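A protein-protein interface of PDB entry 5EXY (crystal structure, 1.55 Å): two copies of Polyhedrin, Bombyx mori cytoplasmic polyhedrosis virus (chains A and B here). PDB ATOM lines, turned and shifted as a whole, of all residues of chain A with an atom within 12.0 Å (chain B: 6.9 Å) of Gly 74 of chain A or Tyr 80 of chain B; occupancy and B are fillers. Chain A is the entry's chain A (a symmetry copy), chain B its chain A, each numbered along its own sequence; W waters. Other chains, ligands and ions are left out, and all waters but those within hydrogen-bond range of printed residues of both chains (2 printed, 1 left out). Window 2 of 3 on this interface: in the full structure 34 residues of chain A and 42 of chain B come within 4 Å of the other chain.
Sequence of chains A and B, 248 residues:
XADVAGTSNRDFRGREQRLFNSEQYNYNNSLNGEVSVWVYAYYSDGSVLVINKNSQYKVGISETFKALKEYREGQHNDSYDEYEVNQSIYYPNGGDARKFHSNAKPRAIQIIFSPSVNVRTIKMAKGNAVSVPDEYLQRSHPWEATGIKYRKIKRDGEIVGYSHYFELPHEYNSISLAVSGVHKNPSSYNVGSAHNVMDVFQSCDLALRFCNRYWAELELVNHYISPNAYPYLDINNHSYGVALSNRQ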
ATOM      1  N   ASP A  45     -18.569 -28.117  -7.472  1.00  0.00           N
ATOM      2  CA  ASP A  45     -19.290 -27.120  -6.672  1.00  0.00           C
ATOM      3  C   ASP A  45     -20.733 -26.926  -7.188  1.00  0.00           C
ATOM      4  O   ASP A  45     -21.424 -26.009  -6.707  1.00  0.00           O
ATOM      5  CB  ASP A  45     -18.545 -25.791  -6.577  1.00  0.00           C
ATOM      6  CG  ASP A  45     -18.354 -25.054  -7.882  1.00  0.00           C
ATOM      7  OD1 ASP A  45     -19.009 -25.424  -8.882  1.00  0.00           O
ATOM      8  OD2 ASP A  45     -17.619 -24.052  -7.893  1.00  0.00           O
ATOM      9  N   SER A  47     -21.627 -25.911 -10.143  1.00  0.00           N
ATOM     10  CA  SER A  47     -21.711 -24.999 -11.242  1.00  0.00           C
ATOM     11  C   SER A  47     -21.530 -25.719 -12.553  1.00  0.00           C
ATOM     12  O   SER A  47     -21.101 -26.878 -12.593  1.00  0.00           O
ATOM     13  CB  SER A  47     -20.758 -23.818 -11.073  1.00  0.00           C
ATOM     14  OG  SER A  47     -19.386 -24.128 -11.159  1.00  0.00           O
ATOM     15  N   GLU A  70     -12.927 -25.111 -14.416  1.00  0.00           N
ATOM     16  CA  GLU A  70     -13.740 -24.066 -13.819  1.00  0.00           C
ATOM     17  C   GLU A  70     -12.969 -22.770 -13.650  1.00  0.00           C
ATOM     18  O   GLU A  70     -11.854 -22.761 -13.140  1.00  0.00           O
ATOM     19  CB  GLU A  70     -14.217 -24.522 -12.443  1.00  0.00           C
ATOM     20  CG  GLU A  70     -15.218 -23.535 -11.879  1.00  0.00           C
ATOM     21  CD  GLU A  70     -15.759 -23.930 -10.529  1.00  0.00           C
ATOM     22  OE1 GLU A  70     -15.230 -24.880  -9.910  1.00  0.00           O
ATOM     23  OE2 GLU A  70     -16.693 -23.237 -10.070  1.00  0.00           O
ATOM     24  N   TYR A  71     -13.599 -21.650 -14.055  1.00  0.00           N
ATOM     25  CA  TYR A  71     -12.999 -20.341 -13.880  1.00  0.00           C
ATOM     26  C   TYR A  71     -14.104 -19.467 -13.311  1.00  0.00           C
ATOM     27  O   TYR A  71     -15.166 -19.337 -13.918  1.00  0.00           O
ATOM     28  CB  TYR A  71     -12.432 -19.756 -15.187  1.00  0.00           C
ATOM     29  CG  TYR A  71     -11.854 -18.375 -14.968  1.00  0.00           C
ATOM     30  CD1 TYR A  71     -10.615 -18.207 -14.363  1.00  0.00           C
ATOM     31  CD2 TYR A  71     -12.562 -17.239 -15.331  1.00  0.00           C
ATOM     32  CE1 TYR A  71     -10.097 -16.938 -14.114  1.00  0.00           C
ATOM     33  CE2 TYR A  71     -12.046 -15.960 -15.105  1.00  0.00           C
ATOM     34  CZ  TYR A  71     -10.821 -15.814 -14.485  1.00  0.00           C
ATOM     35  OH  TYR A  71     -10.335 -14.547 -14.256  1.00  0.00           O
ATOM     36  N   ARG A  72     -13.890 -18.964 -12.108  1.00  0.00           N
ATOM     37  CA  ARG A  72     -14.858 -18.116 -11.403  1.00  0.00           C
ATOM     38  C   ARG A  72     -14.535 -16.656 -11.669  1.00  0.00           C
ATOM     39  O   ARG A  72     -13.592 -16.095 -11.108  1.00  0.00           O
ATOM     40  CB  ARG A  72     -14.849 -18.418  -9.904  1.00  0.00           C
ATOM     41  CG  ARG A  72     -15.009 -19.911  -9.574  1.00  0.00           C
ATOM     42  CD  ARG A  72     -15.289 -20.106  -8.131  1.00  0.00           C
ATOM     43  NE  ARG A  72     -14.207 -19.579  -7.312  1.00  0.00           N
ATOM     44  CZ  ARG A  72     -14.306 -19.306  -6.016  1.00  0.00           C
ATOM     45  NH1 ARG A  72     -15.441 -19.541  -5.362  1.00  0.00           N
ATOM     46  NH2 ARG A  72     -13.260 -18.831  -5.352  1.00  0.00           N
ATOM     47  N   GLU A  73     -15.342 -16.009 -12.536  1.00  0.00           N
ATOM     48  CA  GLU A  73     -15.059 -14.627 -12.894  1.00  0.00           C
ATOM     49  C   GLU A  73     -15.150 -13.720 -11.701  1.00  0.00           C
ATOM     50  O   GLU A  73     -16.121 -13.793 -10.947  1.00  0.00           O
ATOM     51  CB  GLU A  73     -16.032 -14.134 -13.941  1.00  0.00           C
ATOM     52  CG  GLU A  73     -15.879 -14.797 -15.292  1.00  0.00           C
ATOM     53  CD  GLU A  73     -16.853 -14.225 -16.302  1.00  0.00           C
ATOM     54  OE1 GLU A  73     -17.236 -13.041 -16.151  1.00  0.00           O
ATOM     55  OE2 GLU A  73     -17.282 -14.978 -17.205  1.00  0.00           O
ATOM     56  N   GLY A  74     -14.149 -12.869 -11.540  1.00  0.00           N
ATOM     57  CA  GLY A  74     -14.120 -11.910 -10.443  1.00  0.00           C
ATOM     58  C   GLY A  74     -13.890 -12.478  -9.057  1.00  0.00           C
ATOM     59  O   GLY A  74     -14.044 -11.756  -8.073  1.00  0.00           O
ATOM     60  N   GLN A  75     -13.475 -13.760  -8.952  1.00  0.00           N
ATOM     61  CA  GLN A  75     -13.163 -14.389  -7.670  1.00  0.00           C
ATOM     62  C   GLN A  75     -11.790 -15.004  -7.749  1.00  0.00           C
ATOM     63  O   GLN A  75     -11.182 -14.975  -8.822  1.00  0.00           O
ATOM     64  CB  GLN A  75     -14.197 -15.460  -7.324  1.00  0.00           C
ATOM     65  CG  GLN A  75     -15.592 -14.922  -7.095  1.00  0.00           C
ATOM     66  CD  GLN A  75     -16.527 -16.009  -6.660  1.00  0.00           C
ATOM     67  OE1 GLN A  75     -17.074 -16.715  -7.484  1.00  0.00           O
ATOM     68  NE2 GLN A  75     -16.718 -16.185  -5.357  1.00  0.00           N
ATOM     69  N   HIS A  76     -11.255 -15.474  -6.612  1.00  0.00           N
ATOM     70  CA  HIS A  76      -9.922 -16.074  -6.601  1.00  0.00           C
ATOM     71  C   HIS A  76     -10.032 -17.447  -7.213  1.00  0.00           C
ATOM     72  O   HIS A  76     -11.059 -18.110  -7.065  1.00  0.00           O
ATOM     73  CB  HIS A  76      -9.288 -16.131  -5.182  1.00  0.00           C
ATOM     74  CG  HIS A  76      -8.747 -14.807  -4.690  1.00  0.00           C
ATOM     75  ND1 HIS A  76      -7.971 -13.980  -5.495  1.00  0.00           N
ATOM     76  CD2 HIS A  76      -8.782 -14.273  -3.448  1.00  0.00           C
ATOM     77  CE1 HIS A  76      -7.641 -12.940  -4.742  1.00  0.00           C
ATOM     78  NE2 HIS A  76      -8.152 -13.050  -3.513  1.00  0.00           N
ATOM     79  N   ASN A  77      -9.035 -17.838  -8.012  1.00  0.00           N
ATOM     80  CA  ASN A  77      -9.042 -19.126  -8.702  1.00  0.00           C
ATOM     81  C   ASN A  77      -7.753 -19.938  -8.494  1.00  0.00           C
ATOM     82  O   ASN A  77      -7.492 -20.865  -9.269  1.00  0.00           O
ATOM     83  CB  ASN A  77      -9.221 -18.906 -10.203  1.00  0.00           C
ATOM     84  CG  ASN A  77     -10.629 -18.491 -10.557  1.00  0.00           C
ATOM     85  OD1 ASN A  77     -11.540 -19.329 -10.582  1.00  0.00           O
ATOM     86  ND2 ASN A  77     -10.843 -17.207 -10.796  1.00  0.00           N
ATOM     87  N   ASP A  78      -6.978 -19.642  -7.435  1.00  0.00           N
ATOM     88  CA  ASP A  78      -5.734 -20.356  -7.127  1.00  0.00           C
ATOM     89  C   ASP A  78      -4.876 -20.357  -8.422  1.00  0.00           C
ATOM     90  O   ASP A  78      -4.343 -21.393  -8.794  1.00  0.00           O
ATOM     91  CB  ASP A  78      -6.012 -21.822  -6.678  1.00  0.00           C
ATOM     92  CG  ASP A  78      -6.136 -22.176  -5.206  1.00  0.00           C
ATOM     93  OD1 ASP A  78      -6.179 -21.257  -4.372  1.00  0.00           O
ATOM     94  OD2 ASP A  78      -6.201 -23.401  -4.890  1.00  0.00           O
ATOM     95  N   SER A  79      -4.789 -19.228  -9.132  1.00  0.00           N
ATOM     96  CA  SER A  79      -4.210 -19.220 -10.476  1.00  0.00           C
ATOM     97  C   SER A  79      -2.796 -19.760 -10.565  1.00  0.00           C
ATOM     98  O   SER A  79      -2.501 -20.434 -11.535  1.00  0.00           O
ATOM     99  CB  SER A  79      -4.303 -17.847 -11.138  1.00  0.00           C
ATOM    100  OG  SER A  79      -3.491 -16.879 -10.494  1.00  0.00           O
ATOM    101  N   ASN A 212     -20.662 -19.289 -20.685  1.00  0.00           N
ATOM    102  CA  ASN A 212     -20.964 -18.703 -19.398  1.00  0.00           C
ATOM    103  C   ASN A 212     -20.950 -19.776 -18.361  1.00  0.00           C
ATOM    104  O   ASN A 212     -21.275 -20.909 -18.679  1.00  0.00           O
ATOM    105  CB  ASN A 212     -22.339 -18.026 -19.423  1.00  0.00           C
ATOM    106  CG  ASN A 212     -22.610 -17.244 -18.178  1.00  0.00           C
ATOM    107  OD1 ASN A 212     -21.879 -16.331 -17.816  1.00  0.00           O
ATOM    108  ND2 ASN A 212     -23.648 -17.599 -17.474  1.00  0.00           N
ATOM    109  N   ARG A 213     -20.592 -19.433 -17.110  1.00  0.00           N
ATOM    110  CA  ARG A 213     -20.655 -20.391 -15.995  1.00  0.00           C
ATOM    111  C   ARG A 213     -21.857 -20.054 -15.125  1.00  0.00           C
ATOM    112  O   ARG A 213     -21.922 -18.946 -14.578  1.00  0.00           O
ATOM    113  CB  ARG A 213     -19.367 -20.357 -15.167  1.00  0.00           C
ATOM    114  CG  ARG A 213     -19.286 -21.428 -14.073  1.00  0.00           C
ATOM    115  CD  ARG A 213     -18.032 -21.283 -13.188  1.00  0.00           C
ATOM    116  NE  ARG A 213     -18.133 -20.076 -12.357  1.00  0.00           N
ATOM    117  CZ  ARG A 213     -18.616 -20.009 -11.123  1.00  0.00           C
ATOM    118  NH1 ARG A 213     -19.006 -21.115 -10.487  1.00  0.00           N
ATOM    119  NH2 ARG A 213     -18.712 -18.836 -10.507  1.00  0.00           N
ATOM    120  N   TYR A 214     -22.821 -20.970 -15.029  1.00  0.00           N
ATOM    121  CA  TYR A 214     -24.008 -20.821 -14.188  1.00  0.00           C
ATOM    122  C   TYR A 214     -23.741 -21.536 -12.869  1.00  0.00           C
ATOM    123  O   TYR A 214     -22.980 -22.495 -12.825  1.00  0.00           O
ATOM    124  CB  TYR A 214     -25.239 -21.430 -14.868  1.00  0.00           C
ATOM    125  CG  TYR A 214     -25.731 -20.627 -16.047  1.00  0.00           C
ATOM    126  CD1 TYR A 214     -26.519 -19.502 -15.862  1.00  0.00           C
ATOM    127  CD2 TYR A 214     -25.305 -20.918 -17.342  1.00  0.00           C
ATOM    128  CE1 TYR A 214     -26.940 -18.730 -16.938  1.00  0.00           C
ATOM    129  CE2 TYR A 214     -25.692 -20.132 -18.421  1.00  0.00           C
ATOM    130  CZ  TYR A 214     -26.484 -19.016 -18.209  1.00  0.00           C
ATOM    131  OH  TYR A 214     -26.878 -18.162 -19.203  1.00  0.00           O
ATOM    132  N   TRP A 215     -24.298 -21.046 -11.781  1.00  0.00           N
ATOM    133  CA  TRP A 215     -23.977 -21.585 -10.456  1.00  0.00           C
ATOM    134  C   TRP A 215     -24.608 -22.926 -10.132  1.00  0.00           C
ATOM    135  O   TRP A 215     -24.151 -23.608  -9.216  1.00  0.00           O
ATOM    136  CB  TRP A 215     -24.391 -20.614  -9.359  1.00  0.00           C
ATOM    137  CG  TRP A 215     -23.669 -19.297  -9.339  1.00  0.00           C
ATOM    138  CD1 TRP A 215     -22.552 -18.936 -10.040  1.00  0.00           C
ATOM    139  CD2 TRP A 215     -23.956 -18.214  -8.451  1.00  0.00           C
ATOM    140  NE1 TRP A 215     -22.168 -17.659  -9.684  1.00  0.00           N
ATOM    141  CE2 TRP A 215     -23.023 -17.192  -8.718  1.00  0.00           C
ATOM    142  CE3 TRP A 215     -24.971 -17.974  -7.496  1.00  0.00           C
ATOM    143  CZ2 TRP A 215     -23.053 -15.961  -8.047  1.00  0.00           C
ATOM    144  CZ3 TRP A 215     -25.009 -16.744  -6.859  1.00  0.00           C
ATOM    145  CH2 TRP A 215     -24.077 -15.744  -7.166  1.00  0.00           C
ATOM    146  N   ALA A 216     -25.665 -23.303 -10.813  1.00  0.00           N
ATOM    147  CA  ALA A 216     -26.332 -24.564 -10.473  1.00  0.00           C
ATOM    148  C   ALA A 216     -27.070 -25.054 -11.680  1.00  0.00           C
ATOM    149  O   ALA A 216     -27.470 -24.243 -12.501  1.00  0.00           O
ATOM    150  CB  ALA A 216     -27.333 -24.310  -9.366  1.00  0.00           C
ATOM    151  N   GLU A 219     -30.309 -23.136 -12.046  1.00  0.00           N
ATOM    152  CA  GLU A 219     -30.126 -21.835 -12.692  1.00  0.00           C
ATOM    153  C   GLU A 219     -29.976 -21.980 -14.197  1.00  0.00           C
ATOM    154  O   GLU A 219     -30.512 -21.165 -14.961  1.00  0.00           O
ATOM    155  CB  GLU A 219     -28.910 -21.098 -12.114  1.00  0.00           C
ATOM    156  CG  GLU A 219     -28.801 -19.666 -12.576  1.00  0.00           C
ATOM    157  CD  GLU A 219     -27.642 -19.020 -11.849  1.00  0.00           C
ATOM    158  OE1 GLU A 219     -26.478 -19.232 -12.260  1.00  0.00           O
ATOM    159  OE2 GLU A 219     -27.886 -18.517 -10.731  1.00  0.00           O
ATOM    160  N   ASN B  77     -11.565  -3.330 -13.687  1.00  0.00           N
ATOM    161  CA  ASN B  77     -12.685  -3.458 -14.617  1.00  0.00           C
ATOM    162  C   ASN B  77     -13.985  -3.932 -13.945  1.00  0.00           C
ATOM    163  O   ASN B  77     -14.892  -4.394 -14.647  1.00  0.00           O
ATOM    164  CB  ASN B  77     -12.332  -4.459 -15.715  1.00  0.00           C
ATOM    165  CG  ASN B  77     -11.331  -3.901 -16.698  1.00  0.00           C
ATOM    166  OD1 ASN B  77     -11.689  -3.093 -17.565  1.00  0.00           O
ATOM    167  ND2 ASN B  77     -10.070  -4.282 -16.564  1.00  0.00           N
ATOM    168  N   ASP B  78     -14.109  -3.773 -12.616  1.00  0.00           N
ATOM    169  CA  ASP B  78     -15.307  -4.174 -11.868  1.00  0.00           C
ATOM    170  C   ASP B  78     -15.612  -5.648 -12.253  1.00  0.00           C
ATOM    171  O   ASP B  78     -16.756  -5.975 -12.537  1.00  0.00           O
ATOM    172  CB  ASP B  78     -16.528  -3.274 -12.220  1.00  0.00           C
ATOM    173  CG  ASP B  78     -16.869  -2.058 -11.376  1.00  0.00           C
ATOM    174  OD1 ASP B  78     -16.067  -1.695 -10.501  1.00  0.00           O
ATOM    175  OD2 ASP B  78     -17.960  -1.457 -11.608  1.00  0.00           O
ATOM    176  N   SER B  79     -14.597  -6.515 -12.319  1.00  0.00           N
ATOM    177  CA  SER B  79     -14.771  -7.844 -12.908  1.00  0.00           C
ATOM    178  C   SER B  79     -15.866  -8.684 -12.277  1.00  0.00           C
ATOM    179  O   SER B  79     -16.550  -9.375 -13.009  1.00  0.00           O
ATOM    180  CB  SER B  79     -13.461  -8.626 -12.969  1.00  0.00           C
ATOM    181  OG  SER B  79     -12.975  -8.969 -11.681  1.00  0.00           O
ATOM    182  N   TYR B  80     -16.053  -8.636 -10.968  1.00  0.00           N
ATOM    183  CA  TYR B  80     -17.136  -9.421 -10.360  1.00  0.00           C
ATOM    184  C   TYR B  80     -18.464  -8.799 -10.696  1.00  0.00           C
ATOM    185  O   TYR B  80     -19.359  -9.499 -11.175  1.00  0.00           O
ATOM    186  CB  TYR B  80     -16.971  -9.565  -8.843  1.00  0.00           C
ATOM    187  CG  TYR B  80     -17.987 -10.554  -8.338  1.00  0.00           C
ATOM    188  CD1 TYR B  80     -17.823 -11.910  -8.574  1.00  0.00           C
ATOM    189  CD2 TYR B  80     -19.237 -10.127  -7.911  1.00  0.00           C
ATOM    190  CE1 TYR B  80     -18.835 -12.817  -8.316  1.00  0.00           C
ATOM    191  CE2 TYR B  80     -20.275 -11.021  -7.690  1.00  0.00           C
ATOM    192  CZ  TYR B  80     -20.077 -12.369  -7.934  1.00  0.00           C
ATOM    193  OH  TYR B  80     -21.035 -13.320  -7.702  1.00  0.00           O
ATOM    194  N   ASP B  81     -18.609  -7.471 -10.535  1.00  0.00           N
ATOM    195  CA  ASP B  81     -19.912  -6.882 -10.868  1.00  0.00           C
ATOM    196  C   ASP B  81     -20.216  -7.101 -12.350  1.00  0.00           C
ATOM    197  O   ASP B  81     -21.384  -7.180 -12.704  1.00  0.00           O
ATOM    198  CB  ASP B  81     -19.893  -5.379 -10.587  1.00  0.00           C
ATOM    199  CG  ASP B  81     -21.278  -4.772 -10.424  1.00  0.00           C
ATOM    200  OD1 ASP B  81     -22.136  -5.406  -9.780  1.00  0.00           O
ATOM    201  OD2 ASP B  81     -21.504  -3.668 -10.944  1.00  0.00           O
ATOM    202  N   GLU B  82     -19.211  -7.109 -13.229  1.00  0.00           N
ATOM    203  CA  GLU B  82     -19.450  -7.259 -14.648  1.00  0.00           C
ATOM    204  C   GLU B  82     -19.914  -8.684 -15.017  1.00  0.00           C
ATOM    205  O   GLU B  82     -20.670  -8.827 -15.992  1.00  0.00           O
ATOM    206  CB  GLU B  82     -18.274  -6.776 -15.490  1.00  0.00           C
ATOM    207  CG  GLU B  82     -18.184  -5.244 -15.518  1.00  0.00           C
ATOM    208  CD  GLU B  82     -19.358  -4.457 -16.088  1.00  0.00           C
ATOM    209  OE1 GLU B  82     -20.051  -4.963 -17.000  1.00  0.00           O
ATOM    210  OE2 GLU B  82     -19.584  -3.320 -15.621  1.00  0.00           O
ATOM    211  N   TYR B  83     -19.543  -9.710 -14.213  1.00  0.00           N
ATOM    212  CA  TYR B  83     -20.105 -11.061 -14.353  1.00  0.00           C
ATOM    213  C   TYR B  83     -21.591 -10.951 -14.029  1.00  0.00           C
ATOM    214  O   TYR B  83     -22.429 -11.548 -14.727  1.00  0.00           O
ATOM    215  CB  TYR B  83     -19.462 -12.076 -13.375  1.00  0.00           C
ATOM    216  CG  TYR B  83     -20.227 -13.382 -13.253  1.00  0.00           C
ATOM    217  CD1 TYR B  83     -20.018 -14.421 -14.150  1.00  0.00           C
ATOM    218  CD2 TYR B  83     -21.108 -13.605 -12.194  1.00  0.00           C
ATOM    219  CE1 TYR B  83     -20.726 -15.622 -14.049  1.00  0.00           C
ATOM    220  CE2 TYR B  83     -21.824 -14.803 -12.079  1.00  0.00           C
ATOM    221  CZ  TYR B  83     -21.617 -15.817 -13.005  1.00  0.00           C
ATOM    222  OH  TYR B  83     -22.302 -17.017 -12.920  1.00  0.00           O
ATOM    223  N   GLU B  84     -21.942 -10.240 -12.931  1.00  0.00           N
ATOM    224  CA  GLU B  84     -23.341 -10.085 -12.523  1.00  0.00           C
ATOM    225  C   GLU B  84     -24.111  -9.278 -13.554  1.00  0.00           C
ATOM    226  O   GLU B  84     -25.271  -9.580 -13.809  1.00  0.00           O
ATOM    227  CB  GLU B  84     -23.439  -9.417 -11.157  1.00  0.00           C
ATOM    228  CG  GLU B  84     -22.867 -10.242 -10.009  1.00  0.00           C
ATOM    229  CD  GLU B  84     -23.720 -11.444  -9.670  1.00  0.00           C
ATOM    230  OE1 GLU B  84     -24.828 -11.531 -10.239  1.00  0.00           O
ATOM    231  OE2 GLU B  84     -23.251 -12.349  -8.943  1.00  0.00           O
ATOM    232  N   VAL B  85     -23.476  -8.266 -14.157  1.00  0.00           N
ATOM    233  CA  VAL B  85     -24.136  -7.542 -15.241  1.00  0.00           C
ATOM    234  C   VAL B  85     -24.471  -8.533 -16.366  1.00  0.00           C
ATOM    235  O   VAL B  85     -25.577  -8.518 -16.888  1.00  0.00           O
ATOM    236  CB  VAL B  85     -23.221  -6.440 -15.826  1.00  0.00           C
ATOM    237  CG1 VAL B  85     -23.692  -5.955 -17.206  1.00  0.00           C
ATOM    238  CG2 VAL B  85     -23.090  -5.287 -14.865  1.00  0.00           C
ATOM    239  N   ASP B  96     -27.134  -9.957 -10.029  1.00  0.00           N
ATOM    240  CA  ASP B  96     -27.165  -9.181  -8.794  1.00  0.00           C
ATOM    241  C   ASP B  96     -26.148  -8.057  -8.927  1.00  0.00           C
ATOM    242  O   ASP B  96     -25.273  -7.918  -8.081  1.00  0.00           O
ATOM    243  CB  ASP B  96     -26.826 -10.088  -7.592  1.00  0.00           C
ATOM    244  CG  ASP B  96     -27.201  -9.515  -6.235  1.00  0.00           C
ATOM    245  OD1 ASP B  96     -28.015  -8.564  -6.190  1.00  0.00           O
ATOM    246  OD2 ASP B  96     -26.765 -10.078  -5.219  1.00  0.00           O
ATOM    247  N   ALA B  97     -26.232  -7.281 -10.006  1.00  0.00           N
ATOM    248  CA  ALA B  97     -25.252  -6.210 -10.224  1.00  0.00           C
ATOM    249  C   ALA B  97     -25.582  -4.961  -9.416  1.00  0.00           C
ATOM    250  O   ALA B  97     -26.709  -4.794  -8.948  1.00  0.00           O
ATOM    251  CB  ALA B  97     -25.142  -5.852 -11.696  1.00  0.00           C
HETATM  252  O   HOH W   1     -20.186 -15.803  -9.251  1.00  0.00           O
HETATM  253  O   HOH W   2     -24.754 -17.152 -11.928  1.00  0.00           O
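Water W2 lies within hydrogen-bond range of the side-chain hydroxyl (OH) of Tyr 83 of chain B (2.6 Å), the side-chain carboxylate (OE1) of Glu 219 of chain A (2.7 Å) and the indole nitrogen (NE1) of Trp 215 of chain A (3.5 Å). Water W1 bridges the indole nitrogen (NE1) of Trp 215 of chain A (2.7 Å) and the side-chain hydroxyl (OH) of Tyr 80 of chain B (3.0 Å).
Hydrophobic or aromatic side chains of chain B that line the printed part of chain A: Tyr 80 and Tyr 83. Hydrophobic or aromatic side chains of chain A that line the printed part of chain B: Trp 215. Among the printed residues, 8 pairs touch across the chains. Among the printed residues, no Asp or Glu carboxylate lies within 4 Å of a Lys or Arg side-chain nitrogen of the other chain.
Of chain B, only Ser 79 (3.4 Å) and Tyr 80 (3.7 Å) come within 4 Å of Gly 74 of chain A. Tyr 80 of chain B touches just these residues of chain A: Glu 73, Gly 74 and Trp 215. Ser 79 of chain B touches one residue of chain A. No residue of chain A comes within 4 Å of Asp 81 of chain B. Of chain A, only Trp 215 (3.7 Å) comes within 4 Å of Glu 84 of chain B. Of the printed residues of chain A, Tyr 83 of chain B touches Glu 73, Arg 213 and Trp 215. Of the printed residues of chain B, Arg 213 of chain A touches Tyr 83. The nearest printed residue of chain B that does not touch Arg 213 of chain A is Tyr 80 of chain B (6.4 Å).
OH of Tyr 80 of chain B lies within hydrogen-bond range of OE2 of Glu 84 of chain B (2.7 Å). N of Asp 96 of chain B sits at hydrogen-bond distance from OE1 of Glu 84 of chain B (2.8 Å). OG of Ser 47 of chain A sits at hydrogen-bond distance from NH1 of Arg 213 of chain A, at 3.1 Å. The guanidinium group of Arg 213 of chain A lies within salt-bridge range of the side-chain carboxylate of Glu 70 of chain A (3.2 Å). The guanidinium group of Arg 213 of chain A lies within hydrogen-bond range of the backbone carbonyl oxygen of Tyr 71 of chain A (3.4 Å). The side-chain carboxylate of Glu 219 of chain A lies within hydrogen-bond range of the backbone NH of Trp 215 of chain A, at 2.9 Å.
Among the printed residues, merely in contact across the chains: Glu 73 of chain A with Tyr 80 of chain B, Glu 73 of chain A with Tyr 83 of chain B, Gly 74 of chain A with Ser 79 of chain B, Gly 74 of chain A with Tyr 80 of chain B, Trp 215 of chain A with Tyr 80 of chain B and Trp 215 of chain A with Glu 84 of chain B.
Positions printed for both chains: 77, 78 and 79.
The backbone carbonyl oxygen (O) of Arg 213 of chain A sits at hydrogen-bond distance from the side-chain hydroxyl (OH) of Tyr 83 of chain B, at 2.6 Å. The side-chain hydroxyl (OH) of Tyr 83 of chain B is in hydrogen-bond range of the indole nitrogen (NE1) of Trp 215 of chain A (3.3 Å).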
